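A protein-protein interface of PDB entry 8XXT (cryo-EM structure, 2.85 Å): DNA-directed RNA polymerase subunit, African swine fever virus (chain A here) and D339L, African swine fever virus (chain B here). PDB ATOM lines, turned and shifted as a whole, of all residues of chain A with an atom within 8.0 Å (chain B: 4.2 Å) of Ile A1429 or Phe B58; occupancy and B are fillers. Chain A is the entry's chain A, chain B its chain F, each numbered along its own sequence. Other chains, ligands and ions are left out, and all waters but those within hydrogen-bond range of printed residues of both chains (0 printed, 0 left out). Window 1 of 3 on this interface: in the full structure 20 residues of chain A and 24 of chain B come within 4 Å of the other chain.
Of the 13 printed residues of chain A, 5 touch a printed residue of chain B.
Hydrophobic or aromatic side chains of chain A within 4 Å of the printed part of chain B: Tyr A5, Ile A1430 and Met A1431.
Of the 8 printed residues of chain B, 5 touch a printed residue of chain A.
Hydrophobic or aromatic side chains of chain B within 4 Å of the printed part of chain A: Pro B56, Phe B58, Ile B59 and Tyr B69.
Among the printed residues, pairs that only touch across the chains: Tyr A5 with Tyr B69 (3.4 Å), Ile A1430 with Cys B57 (3.5 Å), Ile A1430 with Phe B58 (3.5 Å), Met A1431 with Ile B59 (3.6 Å), Ile A1429 with Phe B58 (3.6 Å), Ile A1430 with Pro B56 (3.8 Å), Glu A1433 with Cys B57 (3.8 Å) and Glu A1433 with Pro B56 (3.9 Å).
The backbone NH (N) of Met A1431 sits at hydrogen-bond distance from the backbone carbonyl oxygen (O) of Cys B57 (2.9 Å).
The backbone NH (N) of Ile B59 lies within hydrogen-bond range of the backbone carbonyl oxygen (O) of Ile A1429, at 3.1 Å.
Of chain B, only Phe B58 (3.6 Å) and Ile B59 (3.1 Å) come within 4 Å of Ile A1429.
Phe B58 touches just these residues of chain A: Ile A1429 and Ile A1430.
Printed residues of chain A within 4 Å of Cys B57: Ile A1430 (3.5 Å), Met A1431 (2.9 Å) and Glu A1433 (3.8 Å).
Of the printed residues of chain A, Ile B59 touches Ile A1429 (3.1 Å) and Met A1431 (3.6 Å).
Printed residues of chain A within 4 Å of Pro B56: Ile A1430 and Glu A1433.
Of the printed residues of chain B, Ile A1430 touches Pro B56 (3.8 Å), Cys B57 (3.5 Å) and Phe B58 (3.5 Å).
Of the printed residues of chain A, Tyr B69 touches Tyr A5 (3.4 Å).
Printed residues of chain B within 4 Å of Met A1431: Cys B57 and Ile B59.
Met A1425 touches none of the printed residues of chain B.
The nearest printed residue of chain B that does not touch Ile A1429 is Cys B57 (4.5 Å).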
ATOM      1  N   TYR A   5     -17.043  12.296  19.387  1.00  0.00           N
ATOM      2  CA  TYR A   5     -17.482  11.611  20.593  1.00  0.00           C
ATOM      3  C   TYR A   5     -18.998  11.481  20.609  1.00  0.00           C
ATOM      4  O   TYR A   5     -19.723  12.421  20.276  1.00  0.00           O
ATOM      5  CB  TYR A   5     -16.993  12.375  21.823  1.00  0.00           C
ATOM      6  CG  TYR A   5     -17.555  11.906  23.140  1.00  0.00           C
ATOM      7  CD1 TYR A   5     -18.716  12.453  23.652  1.00  0.00           C
ATOM      8  CD2 TYR A   5     -16.912  10.931  23.883  1.00  0.00           C
ATOM      9  CE1 TYR A   5     -19.229  12.039  24.852  1.00  0.00           C
ATOM     10  CE2 TYR A   5     -17.420  10.511  25.089  1.00  0.00           C
ATOM     11  CZ  TYR A   5     -18.580  11.070  25.567  1.00  0.00           C
ATOM     12  OH  TYR A   5     -19.101  10.662  26.768  1.00  0.00           O
ATOM     13  N   GLU A   7     -22.486   9.142  22.609  1.00  0.00           N
ATOM     14  CA  GLU A   7     -22.980   8.323  23.705  1.00  0.00           C
ATOM     15  C   GLU A   7     -24.265   7.638  23.279  1.00  0.00           C
ATOM     16  O   GLU A   7     -25.108   8.243  22.615  1.00  0.00           O
ATOM     17  CB  GLU A   7     -23.230   9.161  24.956  1.00  0.00           C
ATOM     18  CG  GLU A   7     -21.999   9.868  25.468  1.00  0.00           C
ATOM     19  CD  GLU A   7     -22.243  10.594  26.767  1.00  0.00           C
ATOM     20  OE1 GLU A   7     -23.387  10.553  27.264  1.00  0.00           O
ATOM     21  OE2 GLU A   7     -21.291  11.207  27.290  1.00  0.00           O
ATOM     22  N   ARG A1421     -24.871   7.720  34.314  1.00  0.00           N
ATOM     23  CA  ARG A1421     -24.960   9.160  34.547  1.00  0.00           C
ATOM     24  C   ARG A1421     -25.548   9.371  35.938  1.00  0.00           C
ATOM     25  O   ARG A1421     -26.749   9.574  36.125  1.00  0.00           O
ATOM     26  CB  ARG A1421     -25.796   9.830  33.464  1.00  0.00           C
ATOM     27  CG  ARG A1421     -26.098  11.296  33.717  1.00  0.00           C
ATOM     28  CD  ARG A1421     -26.724  11.960  32.507  1.00  0.00           C
ATOM     29  NE  ARG A1421     -26.270  11.369  31.256  1.00  0.00           N
ATOM     30  CZ  ARG A1421     -25.471  11.977  30.390  1.00  0.00           C
ATOM     31  NH1 ARG A1421     -25.013  13.199  30.613  1.00  0.00           N
ATOM     32  NH2 ARG A1421     -25.123  11.345  29.273  1.00  0.00           N
ATOM     33  N   THR A1424     -21.154  11.983  40.165  1.00  0.00           N
ATOM     34  CA  THR A1424     -19.990  12.705  39.663  1.00  0.00           C
ATOM     35  C   THR A1424     -20.198  13.159  38.227  1.00  0.00           C
ATOM     36  O   THR A1424     -19.837  14.285  37.875  1.00  0.00           O
ATOM     37  CB  THR A1424     -18.735  11.848  39.781  1.00  0.00           C
ATOM     38  OG1 THR A1424     -18.214  11.954  41.110  1.00  0.00           O
ATOM     39  CG2 THR A1424     -17.676  12.312  38.815  1.00  0.00           C
ATOM     40  N   MET A1425     -20.815  12.322  37.401  1.00  0.00           N
ATOM     41  CA  MET A1425     -21.071  12.660  36.010  1.00  0.00           C
ATOM     42  C   MET A1425     -22.542  12.938  35.743  1.00  0.00           C
ATOM     43  O   MET A1425     -22.992  12.839  34.600  1.00  0.00           O
ATOM     44  CB  MET A1425     -20.556  11.542  35.114  1.00  0.00           C
ATOM     45  CG  MET A1425     -19.178  11.089  35.519  1.00  0.00           C
ATOM     46  SD  MET A1425     -18.300  10.427  34.122  1.00  0.00           S
ATOM     47  CE  MET A1425     -19.469   9.162  33.680  1.00  0.00           C
ATOM     48  N   TYR A1426     -23.302  13.278  36.782  1.00  0.00           N
ATOM     49  CA  TYR A1426     -24.694  13.658  36.582  1.00  0.00           C
ATOM     50  C   TYR A1426     -24.804  14.985  35.850  1.00  0.00           C
ATOM     51  O   TYR A1426     -25.680  15.158  34.995  1.00  0.00           O
ATOM     52  CB  TYR A1426     -25.414  13.731  37.924  1.00  0.00           C
ATOM     53  CG  TYR A1426     -26.916  13.739  37.803  1.00  0.00           C
ATOM     54  CD1 TYR A1426     -27.598  12.623  37.354  1.00  0.00           C
ATOM     55  CD2 TYR A1426     -27.650  14.861  38.141  1.00  0.00           C
ATOM     56  CE1 TYR A1426     -28.968  12.624  37.244  1.00  0.00           C
ATOM     57  CE2 TYR A1426     -29.021  14.870  38.033  1.00  0.00           C
ATOM     58  CZ  TYR A1426     -29.674  13.751  37.584  1.00  0.00           C
ATOM     59  OH  TYR A1426     -31.041  13.753  37.471  1.00  0.00           O
ATOM     60  N   SER A1427     -23.930  15.932  36.168  1.00  0.00           N
ATOM     61  CA  SER A1427     -23.976  17.266  35.590  1.00  0.00           C
ATOM     62  C   SER A1427     -22.902  17.419  34.526  1.00  0.00           C
ATOM     63  O   SER A1427     -21.741  17.060  34.742  1.00  0.00           O
ATOM     64  CB  SER A1427     -23.792  18.334  36.667  1.00  0.00           C
ATOM     65  OG  SER A1427     -24.813  18.255  37.642  1.00  0.00           O
ATOM     66  N   ASP A1428     -23.299  17.951  33.376  1.00  0.00           N
ATOM     67  CA  ASP A1428     -22.352  18.215  32.307  1.00  0.00           C
ATOM     68  C   ASP A1428     -21.406  19.340  32.698  1.00  0.00           C
ATOM     69  O   ASP A1428     -21.773  20.270  33.417  1.00  0.00           O
ATOM     70  CB  ASP A1428     -23.085  18.585  31.022  1.00  0.00           C
ATOM     71  CG  ASP A1428     -23.919  17.449  30.481  1.00  0.00           C
ATOM     72  OD1 ASP A1428     -24.483  16.689  31.293  1.00  0.00           O
ATOM     73  OD2 ASP A1428     -24.012  17.320  29.242  1.00  0.00           O
ATOM     74  N   ILE A1429     -20.174  19.246  32.216  1.00  0.00           N
ATOM     75  CA  ILE A1429     -19.185  20.305  32.352  1.00  0.00           C
ATOM     76  C   ILE A1429     -18.864  20.818  30.959  1.00  0.00           C
ATOM     77  O   ILE A1429     -18.579  20.029  30.052  1.00  0.00           O
ATOM     78  CB  ILE A1429     -17.915  19.812  33.064  1.00  0.00           C
ATOM     79  CG1 ILE A1429     -18.270  19.218  34.422  1.00  0.00           C
ATOM     80  CG2 ILE A1429     -16.934  20.945  33.237  1.00  0.00           C
ATOM     81  CD1 ILE A1429     -19.072  20.137  35.300  1.00  0.00           C
ATOM     82  N   ILE A1430     -18.932  22.131  30.783  1.00  0.00           N
ATOM     83  CA  ILE A1430     -18.617  22.756  29.508  1.00  0.00           C
ATOM     84  C   ILE A1430     -17.551  23.812  29.745  1.00  0.00           C
ATOM     85  O   ILE A1430     -17.398  24.330  30.855  1.00  0.00           O
ATOM     86  CB  ILE A1430     -19.866  23.368  28.835  1.00  0.00           C
ATOM     87  CG1 ILE A1430     -20.247  24.686  29.493  1.00  0.00           C
ATOM     88  CG2 ILE A1430     -21.034  22.416  28.921  1.00  0.00           C
ATOM     89  CD1 ILE A1430     -21.530  25.258  28.975  1.00  0.00           C
ATOM     90  N   MET A1431     -16.792  24.113  28.698  1.00  0.00           N
ATOM     91  CA  MET A1431     -15.755  25.125  28.806  1.00  0.00           C
ATOM     92  C   MET A1431     -16.369  26.518  28.822  1.00  0.00           C
ATOM     93  O   MET A1431     -17.388  26.781  28.179  1.00  0.00           O
ATOM     94  CB  MET A1431     -14.766  25.006  27.652  1.00  0.00           C
ATOM     95  CG  MET A1431     -14.089  23.659  27.552  1.00  0.00           C
ATOM     96  SD  MET A1431     -13.288  23.154  29.079  1.00  0.00           S
ATOM     97  CE  MET A1431     -12.092  24.463  29.288  1.00  0.00           C
ATOM     98  N   ASP A1432     -15.735  27.416  29.573  1.00  0.00           N
ATOM     99  CA  ASP A1432     -16.164  28.812  29.646  1.00  0.00           C
ATOM    100  C   ASP A1432     -15.420  29.588  28.568  1.00  0.00           C
ATOM    101  O   ASP A1432     -14.294  30.044  28.764  1.00  0.00           O
ATOM    102  CB  ASP A1432     -15.911  29.385  31.033  1.00  0.00           C
ATOM    103  CG  ASP A1432     -16.869  30.503  31.384  1.00  0.00           C
ATOM    104  OD1 ASP A1432     -17.529  31.033  30.465  1.00  0.00           O
ATOM    105  OD2 ASP A1432     -16.964  30.857  32.576  1.00  0.00           O
ATOM    106  N   GLU A1433     -16.062  29.734  27.408  1.00  0.00           N
ATOM    107  CA  GLU A1433     -15.444  30.469  26.311  1.00  0.00           C
ATOM    108  C   GLU A1433     -15.211  31.927  26.685  1.00  0.00           C
ATOM    109  O   GLU A1433     -14.152  32.490  26.386  1.00  0.00           O
ATOM    110  CB  GLU A1433     -16.318  30.375  25.062  1.00  0.00           C
ATOM    111  CG  GLU A1433     -16.432  28.980  24.488  1.00  0.00           C
ATOM    112  CD  GLU A1433     -17.769  28.733  23.827  1.00  0.00           C
ATOM    113  OE1 GLU A1433     -18.370  29.699  23.316  1.00  0.00           O
ATOM    114  OE2 GLU A1433     -18.216  27.569  23.805  1.00  0.00           O
ATOM    115  N   SER B  55     -22.301  23.765  19.398  1.00  0.00           N
ATOM    116  CA  SER B  55     -22.608  23.489  20.788  1.00  0.00           C
ATOM    117  C   SER B  55     -21.550  24.099  21.690  1.00  0.00           C
ATOM    118  O   SER B  55     -20.452  24.429  21.240  1.00  0.00           O
ATOM    119  CB  SER B  55     -22.675  21.985  21.020  1.00  0.00           C
ATOM    120  OG  SER B  55     -21.385  21.410  20.953  1.00  0.00           O
ATOM    121  N   PRO B  56     -21.848  24.274  22.974  1.00  0.00           N
ATOM    122  CA  PRO B  56     -20.781  24.596  23.921  1.00  0.00           C
ATOM    123  C   PRO B  56     -19.752  23.480  23.932  1.00  0.00           C
ATOM    124  O   PRO B  56     -20.064  22.317  23.671  1.00  0.00           O
ATOM    125  CB  PRO B  56     -21.515  24.700  25.260  1.00  0.00           C
ATOM    126  CG  PRO B  56     -22.915  25.026  24.890  1.00  0.00           C
ATOM    127  CD  PRO B  56     -23.176  24.310  23.606  1.00  0.00           C
ATOM    128  N   CYS B  57     -18.506  23.842  24.220  1.00  0.00           N
ATOM    129  CA  CYS B  57     -17.445  22.844  24.212  1.00  0.00           C
ATOM    130  C   CYS B  57     -17.588  21.924  25.414  1.00  0.00           C
ATOM    131  O   CYS B  57     -17.033  22.193  26.482  1.00  0.00           O
ATOM    132  CB  CYS B  57     -16.071  23.510  24.207  1.00  0.00           C
ATOM    133  SG  CYS B  57     -14.695  22.350  24.281  1.00  0.00           S
ATOM    134  N   PHE B  58     -18.338  20.837  25.247  1.00  0.00           N
ATOM    135  CA  PHE B  58     -18.581  19.908  26.334  1.00  0.00           C
ATOM    136  C   PHE B  58     -17.284  19.222  26.749  1.00  0.00           C
ATOM    137  O   PHE B  58     -16.222  19.449  26.179  1.00  0.00           O
ATOM    138  CB  PHE B  58     -19.610  18.861  25.924  1.00  0.00           C
ATOM    139  CG  PHE B  58     -20.953  19.428  25.590  1.00  0.00           C
ATOM    140  CD1 PHE B  58     -21.771  19.925  26.580  1.00  0.00           C
ATOM    141  CD2 PHE B  58     -21.401  19.453  24.287  1.00  0.00           C
ATOM    142  CE1 PHE B  58     -23.004  20.442  26.277  1.00  0.00           C
ATOM    143  CE2 PHE B  58     -22.632  19.967  23.981  1.00  0.00           C
ATOM    144  CZ  PHE B  58     -23.434  20.463  24.978  1.00  0.00           C
ATOM    145  N   ILE B  59     -17.385  18.377  27.771  1.00  0.00           N
ATOM    146  CA  ILE B  59     -16.267  17.577  28.256  1.00  0.00           C
ATOM    147  C   ILE B  59     -16.643  16.110  28.117  1.00  0.00           C
ATOM    148  O   ILE B  59     -17.755  15.713  28.481  1.00  0.00           O
ATOM    149  CB  ILE B  59     -15.909  17.923  29.709  1.00  0.00           C
ATOM    150  CG1 ILE B  59     -15.471  19.381  29.821  1.00  0.00           C
ATOM    151  CG2 ILE B  59     -14.806  17.016  30.212  1.00  0.00           C
ATOM    152  CD1 ILE B  59     -14.450  19.787  28.808  1.00  0.00           C
ATOM    153  N   GLY B  68     -12.710  17.583  25.152  1.00  0.00           N
ATOM    154  CA  GLY B  68     -14.056  17.961  24.801  1.00  0.00           C
ATOM    155  C   GLY B  68     -14.367  17.572  23.367  1.00  0.00           C
ATOM    156  O   GLY B  68     -13.484  17.231  22.585  1.00  0.00           O
ATOM    157  N   TYR B  69     -15.653  17.608  23.028  1.00  0.00           N
ATOM    158  CA  TYR B  69     -16.041  17.276  21.664  1.00  0.00           C
ATOM    159  C   TYR B  69     -16.673  18.447  20.925  1.00  0.00           C
ATOM    160  O   TYR B  69     -16.152  18.847  19.880  1.00  0.00           O
ATOM    161  CB  TYR B  69     -16.965  16.049  21.634  1.00  0.00           C
ATOM    162  CG  TYR B  69     -18.063  15.993  22.666  1.00  0.00           C
ATOM    163  CD1 TYR B  69     -17.789  15.673  23.984  1.00  0.00           C
ATOM    164  CD2 TYR B  69     -19.383  16.202  22.306  1.00  0.00           C
ATOM    165  CE1 TYR B  69     -18.790  15.601  24.916  1.00  0.00           C
ATOM    166  CE2 TYR B  69     -20.387  16.128  23.233  1.00  0.00           C
ATOM    167  CZ  TYR B  69     -20.085  15.826  24.535  1.00  0.00           C
ATOM    168  OH  TYR B  69     -21.084  15.752  25.471  1.00  0.00           O
ATOM    169  N   HIS B  71     -20.388  19.890  19.236  1.00  0.00           N
ATOM    170  CA  HIS B  71     -21.057  19.629  17.973  1.00  0.00           C
ATOM    171  C   HIS B  71     -21.002  20.874  17.101  1.00  0.00           C
ATOM    172  O   HIS B  71     -21.107  21.996  17.597  1.00  0.00           O
ATOM    173  CB  HIS B  71     -22.511  19.224  18.204  1.00  0.00           C
ATOM    174  CG  HIS B  71     -22.688  18.163  19.244  1.00  0.00           C
ATOM    175  ND1 HIS B  71     -22.079  16.932  19.160  1.00  0.00           N
ATOM    176  CD2 HIS B  71     -23.411  18.148  20.386  1.00  0.00           C
ATOM    177  CE1 HIS B  71     -22.416  16.204  20.208  1.00  0.00           C
ATOM    178  NE2 HIS B  71     -23.224  16.919  20.968  1.00  0.00           N
